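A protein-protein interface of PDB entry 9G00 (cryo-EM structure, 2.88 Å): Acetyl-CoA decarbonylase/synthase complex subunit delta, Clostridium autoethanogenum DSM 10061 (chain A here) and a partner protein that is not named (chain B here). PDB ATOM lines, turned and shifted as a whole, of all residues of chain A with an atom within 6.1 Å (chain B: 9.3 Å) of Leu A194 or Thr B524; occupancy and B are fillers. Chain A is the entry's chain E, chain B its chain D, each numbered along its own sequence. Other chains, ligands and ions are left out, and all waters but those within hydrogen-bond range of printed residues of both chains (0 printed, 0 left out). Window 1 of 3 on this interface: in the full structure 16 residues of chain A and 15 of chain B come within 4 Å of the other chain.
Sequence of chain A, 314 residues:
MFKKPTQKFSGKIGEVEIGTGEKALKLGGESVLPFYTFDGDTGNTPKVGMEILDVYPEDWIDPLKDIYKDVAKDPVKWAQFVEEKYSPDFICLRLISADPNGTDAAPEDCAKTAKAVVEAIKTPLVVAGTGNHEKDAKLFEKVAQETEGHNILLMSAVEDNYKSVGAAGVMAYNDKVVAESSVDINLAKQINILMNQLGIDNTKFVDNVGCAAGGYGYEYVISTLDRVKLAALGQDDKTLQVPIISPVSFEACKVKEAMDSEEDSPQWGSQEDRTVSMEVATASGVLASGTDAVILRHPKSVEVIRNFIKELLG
The guanidinium group of Arg B227 lies within hydrogen-bond range of the backbone carbonyl oxygen of Leu A198, at 3.4 Å.
NE2 of Gln A190 is in hydrogen-bond range of O of Thr B524 (3.4 Å).
The backbone carbonyl oxygen (O) of Gln A197 is in hydrogen-bond range of the guanidinium group (NH2) of Arg B227 (3.1 Å).
Among the printed residues, merely in contact across the chains: Leu A198 with Val B128 and Leu A194 with Thr B524.
Printed residues of chain B within 4 Å of Leu A194: Thr B524.
Thr B524 touches just these residues of chain A: Gln A190 (3.4 Å) and Leu A194 (3.8 Å).
No residue of chain B comes within 4 Å of Ile A193.
Of the printed residues of chain B, Gln A197 touches Arg B227 (3.1 Å).
Printed residues of chain A within 4 Å of Arg B227: Gln A197 and Leu A198.
The nearest residue of chain B that does not touch Leu A194 is Asn B522 (6.6 Å).
The nearest residue of chain A that does not touch Thr B524 is Ile A193 (4.2 Å).
Of the 15 printed residues of chain B, 3 touch a printed residue of chain A.
Hydrophobic or aromatic side chains of chain B that line the printed part of chain A: Val B128.
Hydrophobic or aromatic side chains of chain A within 4 Å of the printed part of chain B: Leu A194 and Leu A198.
Among the printed residues, 5 pairs touch across the chains.
Among the printed residues, no Asp or Glu carboxylate lies within 4 Å of a Lys or Arg side-chain nitrogen of the other chain.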
ATOM      1  N   GLU A 159     -10.103 -21.915  -2.523  1.00  0.00           N
ATOM      2  CA  GLU A 159     -10.542 -21.779  -1.138  1.00  0.00           C
ATOM      3  C   GLU A 159     -11.675 -22.740  -0.794  1.00  0.00           C
ATOM      4  O   GLU A 159     -11.797 -23.172   0.357  1.00  0.00           O
ATOM      5  CB  GLU A 159     -10.990 -20.341  -0.877  1.00  0.00           C
ATOM      6  CG  GLU A 159     -11.282 -20.043   0.585  1.00  0.00           C
ATOM      7  CD  GLU A 159     -12.257 -18.901   0.763  1.00  0.00           C
ATOM      8  OE1 GLU A 159     -12.755 -18.374  -0.252  1.00  0.00           O
ATOM      9  OE2 GLU A 159     -12.531 -18.535   1.924  1.00  0.00           O
ATOM     10  N   TYR A 162      -9.920 -26.351  -0.551  1.00  0.00           N
ATOM     11  CA  TYR A 162      -8.552 -26.417  -0.046  1.00  0.00           C
ATOM     12  C   TYR A 162      -8.449 -27.383   1.128  1.00  0.00           C
ATOM     13  O   TYR A 162      -7.432 -28.068   1.287  1.00  0.00           O
ATOM     14  CB  TYR A 162      -8.066 -25.025   0.350  1.00  0.00           C
ATOM     15  CG  TYR A 162      -8.294 -24.669   1.799  1.00  0.00           C
ATOM     16  CD1 TYR A 162      -9.501 -24.137   2.222  1.00  0.00           C
ATOM     17  CD2 TYR A 162      -7.296 -24.857   2.741  1.00  0.00           C
ATOM     18  CE1 TYR A 162      -9.709 -23.809   3.543  1.00  0.00           C
ATOM     19  CE2 TYR A 162      -7.495 -24.533   4.060  1.00  0.00           C
ATOM     20  CZ  TYR A 162      -8.702 -24.011   4.457  1.00  0.00           C
ATOM     21  OH  TYR A 162      -8.894 -23.687   5.779  1.00  0.00           O
ATOM     22  N   LYS A 189      -3.067 -13.899  -0.820  1.00  0.00           N
ATOM     23  CA  LYS A 189      -2.613 -13.855   0.562  1.00  0.00           C
ATOM     24  C   LYS A 189      -3.567 -14.610   1.482  1.00  0.00           C
ATOM     25  O   LYS A 189      -3.130 -15.254   2.440  1.00  0.00           O
ATOM     26  CB  LYS A 189      -2.465 -12.398   0.993  1.00  0.00           C
ATOM     27  CG  LYS A 189      -1.833 -12.185   2.348  1.00  0.00           C
ATOM     28  CD  LYS A 189      -1.418 -10.731   2.520  1.00  0.00           C
ATOM     29  CE  LYS A 189      -1.067 -10.400   3.961  1.00  0.00           C
ATOM     30  NZ  LYS A 189      -2.241 -10.498   4.877  1.00  0.00           N
ATOM     31  N   GLN A 190      -4.870 -14.561   1.196  1.00  0.00           N
ATOM     32  CA  GLN A 190      -5.842 -15.245   2.046  1.00  0.00           C
ATOM     33  C   GLN A 190      -5.700 -16.757   1.948  1.00  0.00           C
ATOM     34  O   GLN A 190      -5.662 -17.453   2.968  1.00  0.00           O
ATOM     35  CB  GLN A 190      -7.262 -14.826   1.665  1.00  0.00           C
ATOM     36  CG  GLN A 190      -8.347 -15.491   2.504  1.00  0.00           C
ATOM     37  CD  GLN A 190      -9.733 -15.264   1.948  1.00  0.00           C
ATOM     38  OE1 GLN A 190      -9.960 -15.391   0.747  1.00  0.00           O
ATOM     39  NE2 GLN A 190     -10.671 -14.924   2.820  1.00  0.00           N
ATOM     40  N   ILE A 191      -5.629 -17.288   0.727  1.00  0.00           N
ATOM     41  CA  ILE A 191      -5.590 -18.738   0.563  1.00  0.00           C
ATOM     42  C   ILE A 191      -4.315 -19.305   1.172  1.00  0.00           C
ATOM     43  O   ILE A 191      -4.316 -20.408   1.725  1.00  0.00           O
ATOM     44  CB  ILE A 191      -5.738 -19.121  -0.923  1.00  0.00           C
ATOM     45  CG1 ILE A 191      -5.689 -20.639  -1.097  1.00  0.00           C
ATOM     46  CG2 ILE A 191      -4.652 -18.483  -1.759  1.00  0.00           C
ATOM     47  CD1 ILE A 191      -6.785 -21.382  -0.377  1.00  0.00           C
ATOM     48  N   ASN A 192      -3.206 -18.571   1.070  1.00  0.00           N
ATOM     49  CA  ASN A 192      -1.966 -19.031   1.686  1.00  0.00           C
ATOM     50  C   ASN A 192      -2.096 -19.094   3.201  1.00  0.00           C
ATOM     51  O   ASN A 192      -1.563 -20.008   3.839  1.00  0.00           O
ATOM     52  CB  ASN A 192      -0.808 -18.116   1.297  1.00  0.00           C
ATOM     53  CG  ASN A 192      -0.509 -18.155  -0.180  1.00  0.00           C
ATOM     54  OD1 ASN A 192      -0.866 -19.104  -0.873  1.00  0.00           O
ATOM     55  ND2 ASN A 192       0.160 -17.125  -0.672  1.00  0.00           N
ATOM     56  N   ILE A 193      -2.779 -18.116   3.799  1.00  0.00           N
ATOM     57  CA  ILE A 193      -2.978 -18.129   5.246  1.00  0.00           C
ATOM     58  C   ILE A 193      -3.797 -19.342   5.659  1.00  0.00           C
ATOM     59  O   ILE A 193      -3.502 -19.997   6.664  1.00  0.00           O
ATOM     60  CB  ILE A 193      -3.631 -16.814   5.711  1.00  0.00           C
ATOM     61  CG1 ILE A 193      -2.627 -15.669   5.580  1.00  0.00           C
ATOM     62  CG2 ILE A 193      -4.107 -16.931   7.150  1.00  0.00           C
ATOM     63  CD1 ILE A 193      -3.165 -14.309   5.956  1.00  0.00           C
ATOM     64  N   LEU A 194      -4.841 -19.660   4.893  1.00  0.00           N
ATOM     65  CA  LEU A 194      -5.670 -20.813   5.224  1.00  0.00           C
ATOM     66  C   LEU A 194      -4.869 -22.107   5.163  1.00  0.00           C
ATOM     67  O   LEU A 194      -5.050 -22.995   6.002  1.00  0.00           O
ATOM     68  CB  LEU A 194      -6.871 -20.876   4.285  1.00  0.00           C
ATOM     69  CG  LEU A 194      -7.827 -19.687   4.362  1.00  0.00           C
ATOM     70  CD1 LEU A 194      -8.981 -19.867   3.399  1.00  0.00           C
ATOM     71  CD2 LEU A 194      -8.347 -19.509   5.772  1.00  0.00           C
ATOM     72  N   MET A 195      -3.988 -22.241   4.171  1.00  0.00           N
ATOM     73  CA  MET A 195      -3.134 -23.422   4.107  1.00  0.00           C
ATOM     74  C   MET A 195      -2.198 -23.483   5.306  1.00  0.00           C
ATOM     75  O   MET A 195      -1.977 -24.556   5.876  1.00  0.00           O
ATOM     76  CB  MET A 195      -2.325 -23.421   2.810  1.00  0.00           C
ATOM     77  CG  MET A 195      -3.162 -23.361   1.548  1.00  0.00           C
ATOM     78  SD  MET A 195      -4.168 -24.824   1.261  1.00  0.00           S
ATOM     79  CE  MET A 195      -2.918 -26.013   0.793  1.00  0.00           C
ATOM     80  N   ASN A 196      -1.628 -22.343   5.696  1.00  0.00           N
ATOM     81  CA  ASN A 196      -0.720 -22.325   6.837  1.00  0.00           C
ATOM     82  C   ASN A 196      -1.444 -22.674   8.130  1.00  0.00           C
ATOM     83  O   ASN A 196      -0.910 -23.410   8.966  1.00  0.00           O
ATOM     84  CB  ASN A 196      -0.053 -20.958   6.950  1.00  0.00           C
ATOM     85  CG  ASN A 196       0.897 -20.687   5.810  1.00  0.00           C
ATOM     86  OD1 ASN A 196       0.777 -19.684   5.109  1.00  0.00           O
ATOM     87  ND2 ASN A 196       1.849 -21.587   5.614  1.00  0.00           N
ATOM     88  N   GLN A 197      -2.654 -22.148   8.319  1.00  0.00           N
ATOM     89  CA  GLN A 197      -3.407 -22.471   9.524  1.00  0.00           C
ATOM     90  C   GLN A 197      -3.805 -23.940   9.552  1.00  0.00           C
ATOM     91  O   GLN A 197      -3.861 -24.546  10.627  1.00  0.00           O
ATOM     92  CB  GLN A 197      -4.641 -21.579   9.623  1.00  0.00           C
ATOM     93  CG  GLN A 197      -4.309 -20.113   9.834  1.00  0.00           C
ATOM     94  CD  GLN A 197      -5.538 -19.233   9.818  1.00  0.00           C
ATOM     95  OE1 GLN A 197      -6.640 -19.693   9.527  1.00  0.00           O
ATOM     96  NE2 GLN A 197      -5.354 -17.957  10.133  1.00  0.00           N
ATOM     97  N   LEU A 198      -4.073 -24.527   8.386  1.00  0.00           N
ATOM     98  CA  LEU A 198      -4.428 -25.938   8.326  1.00  0.00           C
ATOM     99  C   LEU A 198      -3.266 -26.844   8.709  1.00  0.00           C
ATOM    100  O   LEU A 198      -3.488 -28.022   9.006  1.00  0.00           O
ATOM    101  CB  LEU A 198      -4.918 -26.290   6.922  1.00  0.00           C
ATOM    102  CG  LEU A 198      -5.500 -27.690   6.739  1.00  0.00           C
ATOM    103  CD1 LEU A 198      -6.663 -27.915   7.686  1.00  0.00           C
ATOM    104  CD2 LEU A 198      -5.938 -27.885   5.299  1.00  0.00           C
ATOM    105  N   GLY A 199      -2.044 -26.332   8.697  1.00  0.00           N
ATOM    106  CA  GLY A 199      -0.868 -27.105   9.012  1.00  0.00           C
ATOM    107  C   GLY A 199       0.085 -27.339   7.859  1.00  0.00           C
ATOM    108  O   GLY A 199       0.935 -28.233   7.959  1.00  0.00           O
ATOM    109  N   VAL B 128     -10.065 -34.104   8.718  1.00  0.00           N
ATOM    110  CA  VAL B 128      -9.638 -32.721   8.539  1.00  0.00           C
ATOM    111  C   VAL B 128     -10.765 -31.885   7.954  1.00  0.00           C
ATOM    112  O   VAL B 128     -10.999 -30.748   8.380  1.00  0.00           O
ATOM    113  CB  VAL B 128      -8.372 -32.661   7.668  1.00  0.00           C
ATOM    114  CG1 VAL B 128      -7.949 -31.213   7.439  1.00  0.00           C
ATOM    115  CG2 VAL B 128      -7.241 -33.449   8.327  1.00  0.00           C
ATOM    116  N   ARG B 227      -7.028 -30.779  17.741  1.00  0.00           N
ATOM    117  CA  ARG B 227      -7.281 -31.241  16.384  1.00  0.00           C
ATOM    118  C   ARG B 227      -8.097 -32.525  16.288  1.00  0.00           C
ATOM    119  O   ARG B 227      -8.788 -32.712  15.284  1.00  0.00           O
ATOM    120  CB  ARG B 227      -5.949 -31.466  15.658  1.00  0.00           C
ATOM    121  CG  ARG B 227      -5.069 -30.222  15.618  1.00  0.00           C
ATOM    122  CD  ARG B 227      -5.646 -29.182  14.658  1.00  0.00           C
ATOM    123  NE  ARG B 227      -4.585 -28.575  13.865  1.00  0.00           N
ATOM    124  CZ  ARG B 227      -4.769 -27.668  12.916  1.00  0.00           C
ATOM    125  NH1 ARG B 227      -5.973 -27.222  12.607  1.00  0.00           N
ATOM    126  NH2 ARG B 227      -3.711 -27.191  12.256  1.00  0.00           N
ATOM    127  N   SER B 484      -9.612  -2.026   9.843  1.00  0.00           N
ATOM    128  CA  SER B 484      -9.022  -1.689   8.557  1.00  0.00           C
ATOM    129  C   SER B 484      -9.619  -2.585   7.485  1.00  0.00           C
ATOM    130  O   SER B 484      -9.645  -3.808   7.638  1.00  0.00           O
ATOM    131  CB  SER B 484      -7.501  -1.843   8.590  1.00  0.00           C
ATOM    132  OG  SER B 484      -7.125  -3.151   8.981  1.00  0.00           O
ATOM    133  N   ASN B 486      -9.657  -3.529   3.249  1.00  0.00           N
ATOM    134  CA  ASN B 486      -8.824  -3.468   2.050  1.00  0.00           C
ATOM    135  C   ASN B 486      -9.499  -4.179   0.891  1.00  0.00           C
ATOM    136  O   ASN B 486      -8.850  -4.874   0.105  1.00  0.00           O
ATOM    137  CB  ASN B 486      -7.445  -4.068   2.308  1.00  0.00           C
ATOM    138  CG  ASN B 486      -7.512  -5.527   2.664  1.00  0.00           C
ATOM    139  OD1 ASN B 486      -8.564  -6.033   3.042  1.00  0.00           O
ATOM    140  ND2 ASN B 486      -6.389  -6.217   2.550  1.00  0.00           N
ATOM    141  N   THR B 518     -17.642  -8.430  10.593  1.00  0.00           N
ATOM    142  CA  THR B 518     -16.922  -9.051   9.486  1.00  0.00           C
ATOM    143  C   THR B 518     -15.676  -9.764   9.987  1.00  0.00           C
ATOM    144  O   THR B 518     -15.357 -10.870   9.537  1.00  0.00           O
ATOM    145  CB  THR B 518     -16.546  -8.000   8.444  1.00  0.00           C
ATOM    146  OG1 THR B 518     -17.727  -7.340   7.973  1.00  0.00           O
ATOM    147  CG2 THR B 518     -15.826  -8.640   7.267  1.00  0.00           C
ATOM    148  N   LEU B 519     -14.960  -9.146  10.923  1.00  0.00           N
ATOM    149  CA  LEU B 519     -13.776  -9.785  11.482  1.00  0.00           C
ATOM    150  C   LEU B 519     -14.143 -11.061  12.226  1.00  0.00           C
ATOM    151  O   LEU B 519     -13.396 -12.045  12.188  1.00  0.00           O
ATOM    152  CB  LEU B 519     -13.048  -8.809  12.404  1.00  0.00           C
ATOM    153  CG  LEU B 519     -11.857  -9.373  13.180  1.00  0.00           C
ATOM    154  CD1 LEU B 519     -10.812  -9.943  12.240  1.00  0.00           C
ATOM    155  CD2 LEU B 519     -11.254  -8.301  14.061  1.00  0.00           C
ATOM    156  N   GLU B 520     -15.278 -11.063  12.925  1.00  0.00           N
ATOM    157  CA  GLU B 520     -15.669 -12.242  13.691  1.00  0.00           C
ATOM    158  C   GLU B 520     -16.118 -13.377  12.778  1.00  0.00           C
ATOM    159  O   GLU B 520     -15.722 -14.533  12.967  1.00  0.00           O
ATOM    160  CB  GLU B 520     -16.780 -11.880  14.674  1.00  0.00           C
ATOM    161  CG  GLU B 520     -17.125 -12.997  15.642  1.00  0.00           C
ATOM    162  CD  GLU B 520     -15.987 -13.314  16.586  1.00  0.00           C
ATOM    163  OE1 GLU B 520     -15.120 -12.437  16.789  1.00  0.00           O
ATOM    164  OE2 GLU B 520     -15.953 -14.440  17.123  1.00  0.00           O
ATOM    165  N   LEU B 521     -16.954 -13.070  11.786  1.00  0.00           N
ATOM    166  CA  LEU B 521     -17.429 -14.109  10.877  1.00  0.00           C
ATOM    167  C   LEU B 521     -16.320 -14.601   9.958  1.00  0.00           C
ATOM    168  O   LEU B 521     -16.229 -15.802   9.676  1.00  0.00           O
ATOM    169  CB  LEU B 521     -18.599 -13.585  10.050  1.00  0.00           C
ATOM    170  CG  LEU B 521     -19.992 -13.777  10.642  1.00  0.00           C
ATOM    171  CD1 LEU B 521     -20.204 -12.912  11.868  1.00  0.00           C
ATOM    172  CD2 LEU B 521     -21.025 -13.469   9.584  1.00  0.00           C
ATOM    173  N   ASN B 522     -15.476 -13.695   9.476  1.00  0.00           N
ATOM    174  CA  ASN B 522     -14.422 -14.016   8.517  1.00  0.00           C
ATOM    175  C   ASN B 522     -13.100 -13.506   9.076  1.00  0.00           C
ATOM    176  O   ASN B 522     -12.643 -12.413   8.720  1.00  0.00           O
ATOM    177  CB  ASN B 522     -14.727 -13.397   7.154  1.00  0.00           C
ATOM    178  CG  ASN B 522     -14.033 -14.112   6.027  1.00  0.00           C
ATOM    179  OD1 ASN B 522     -13.106 -14.889   6.249  1.00  0.00           O
ATOM    180  ND2 ASN B 522     -14.477 -13.858   4.802  1.00  0.00           N
ATOM    181  N   PRO B 523     -12.448 -14.284   9.944  1.00  0.00           N
ATOM    182  CA  PRO B 523     -11.209 -13.791  10.567  1.00  0.00           C
ATOM    183  C   PRO B 523     -10.123 -13.431   9.574  1.00  0.00           C
ATOM    184  O   PRO B 523      -9.324 -12.527   9.847  1.00  0.00           O
ATOM    185  CB  PRO B 523     -10.784 -14.959  11.469  1.00  0.00           C
ATOM    186  CG  PRO B 523     -11.484 -16.141  10.930  1.00  0.00           C
ATOM    187  CD  PRO B 523     -12.782 -15.642  10.399  1.00  0.00           C
ATOM    188  N   THR B 524     -10.059 -14.114   8.435  1.00  0.00           N
ATOM    189  CA  THR B 524      -9.067 -13.836   7.407  1.00  0.00           C
ATOM    190  C   THR B 524      -9.628 -12.966   6.285  1.00  0.00           C
ATOM    191  O   THR B 524      -9.088 -12.969   5.175  1.00  0.00           O
ATOM    192  CB  THR B 524      -8.526 -15.149   6.844  1.00  0.00           C
ATOM    193  OG1 THR B 524      -7.514 -14.882   5.868  1.00  0.00           O
ATOM    194  CG2 THR B 524      -9.643 -15.950   6.206  1.00  0.00           C
ATOM    195  N   GLY B 525     -10.694 -12.221   6.559  1.00  0.00           N
ATOM    196  CA  GLY B 525     -11.360 -11.428   5.554  1.00  0.00           C
ATOM    197  C   GLY B 525     -10.757 -10.048   5.395  1.00  0.00           C
ATOM    198  O   GLY B 525      -9.624  -9.786   5.807  1.00  0.00           O
ATOM    199  N   PRO B 526     -11.506  -9.141   4.763  1.00  0.00           N
ATOM    200  CA  PRO B 526     -10.965  -7.798   4.504  1.00  0.00           C
ATOM    201  C   PRO B 526     -10.851  -6.922   5.736  1.00  0.00           C
ATOM    202  O   PRO B 526     -10.035  -5.993   5.731  1.00  0.00           O
ATOM    203  CB  PRO B 526     -11.967  -7.204   3.507  1.00  0.00           C
ATOM    204  CG  PRO B 526     -12.782  -8.351   3.030  1.00  0.00           C
ATOM    205  CD  PRO B 526     -12.822  -9.321   4.141  1.00  0.00           C
ATOM    206  N   CYS B 527     -11.628  -7.176   6.784  1.00  0.00           N
ATOM    207  CA  CYS B 527     -11.651  -6.320   7.962  1.00  0.00           C
ATOM    208  C   CYS B 527     -10.835  -6.961   9.075  1.00  0.00           C
ATOM    209  O   CYS B 527     -11.075  -8.115   9.438  1.00  0.00           O
ATOM    210  CB  CYS B 527     -13.086  -6.078   8.423  1.00  0.00           C
ATOM    211  SG  CYS B 527     -14.106  -5.247   7.190  1.00  0.00           S
ATOM    212  N   GLN B 528      -9.868  -6.214   9.601  1.00  0.00           N
ATOM    213  CA  GLN B 528      -8.993  -6.690  10.661  1.00  0.00           C
ATOM    214  C   GLN B 528      -8.895  -5.635  11.752  1.00  0.00           C
ATOM    215  O   GLN B 528      -9.026  -4.438  11.491  1.00  0.00           O
ATOM    216  CB  GLN B 528      -7.598  -7.016  10.136  1.00  0.00           C
ATOM    217  CG  GLN B 528      -7.589  -8.017   9.002  1.00  0.00           C
ATOM    218  CD  GLN B 528      -8.138  -9.365   9.408  1.00  0.00           C
ATOM    219  OE1 GLN B 528      -7.797  -9.897  10.463  1.00  0.00           O
ATOM    220  NE2 GLN B 528      -9.000  -9.926   8.571  1.00  0.00           N
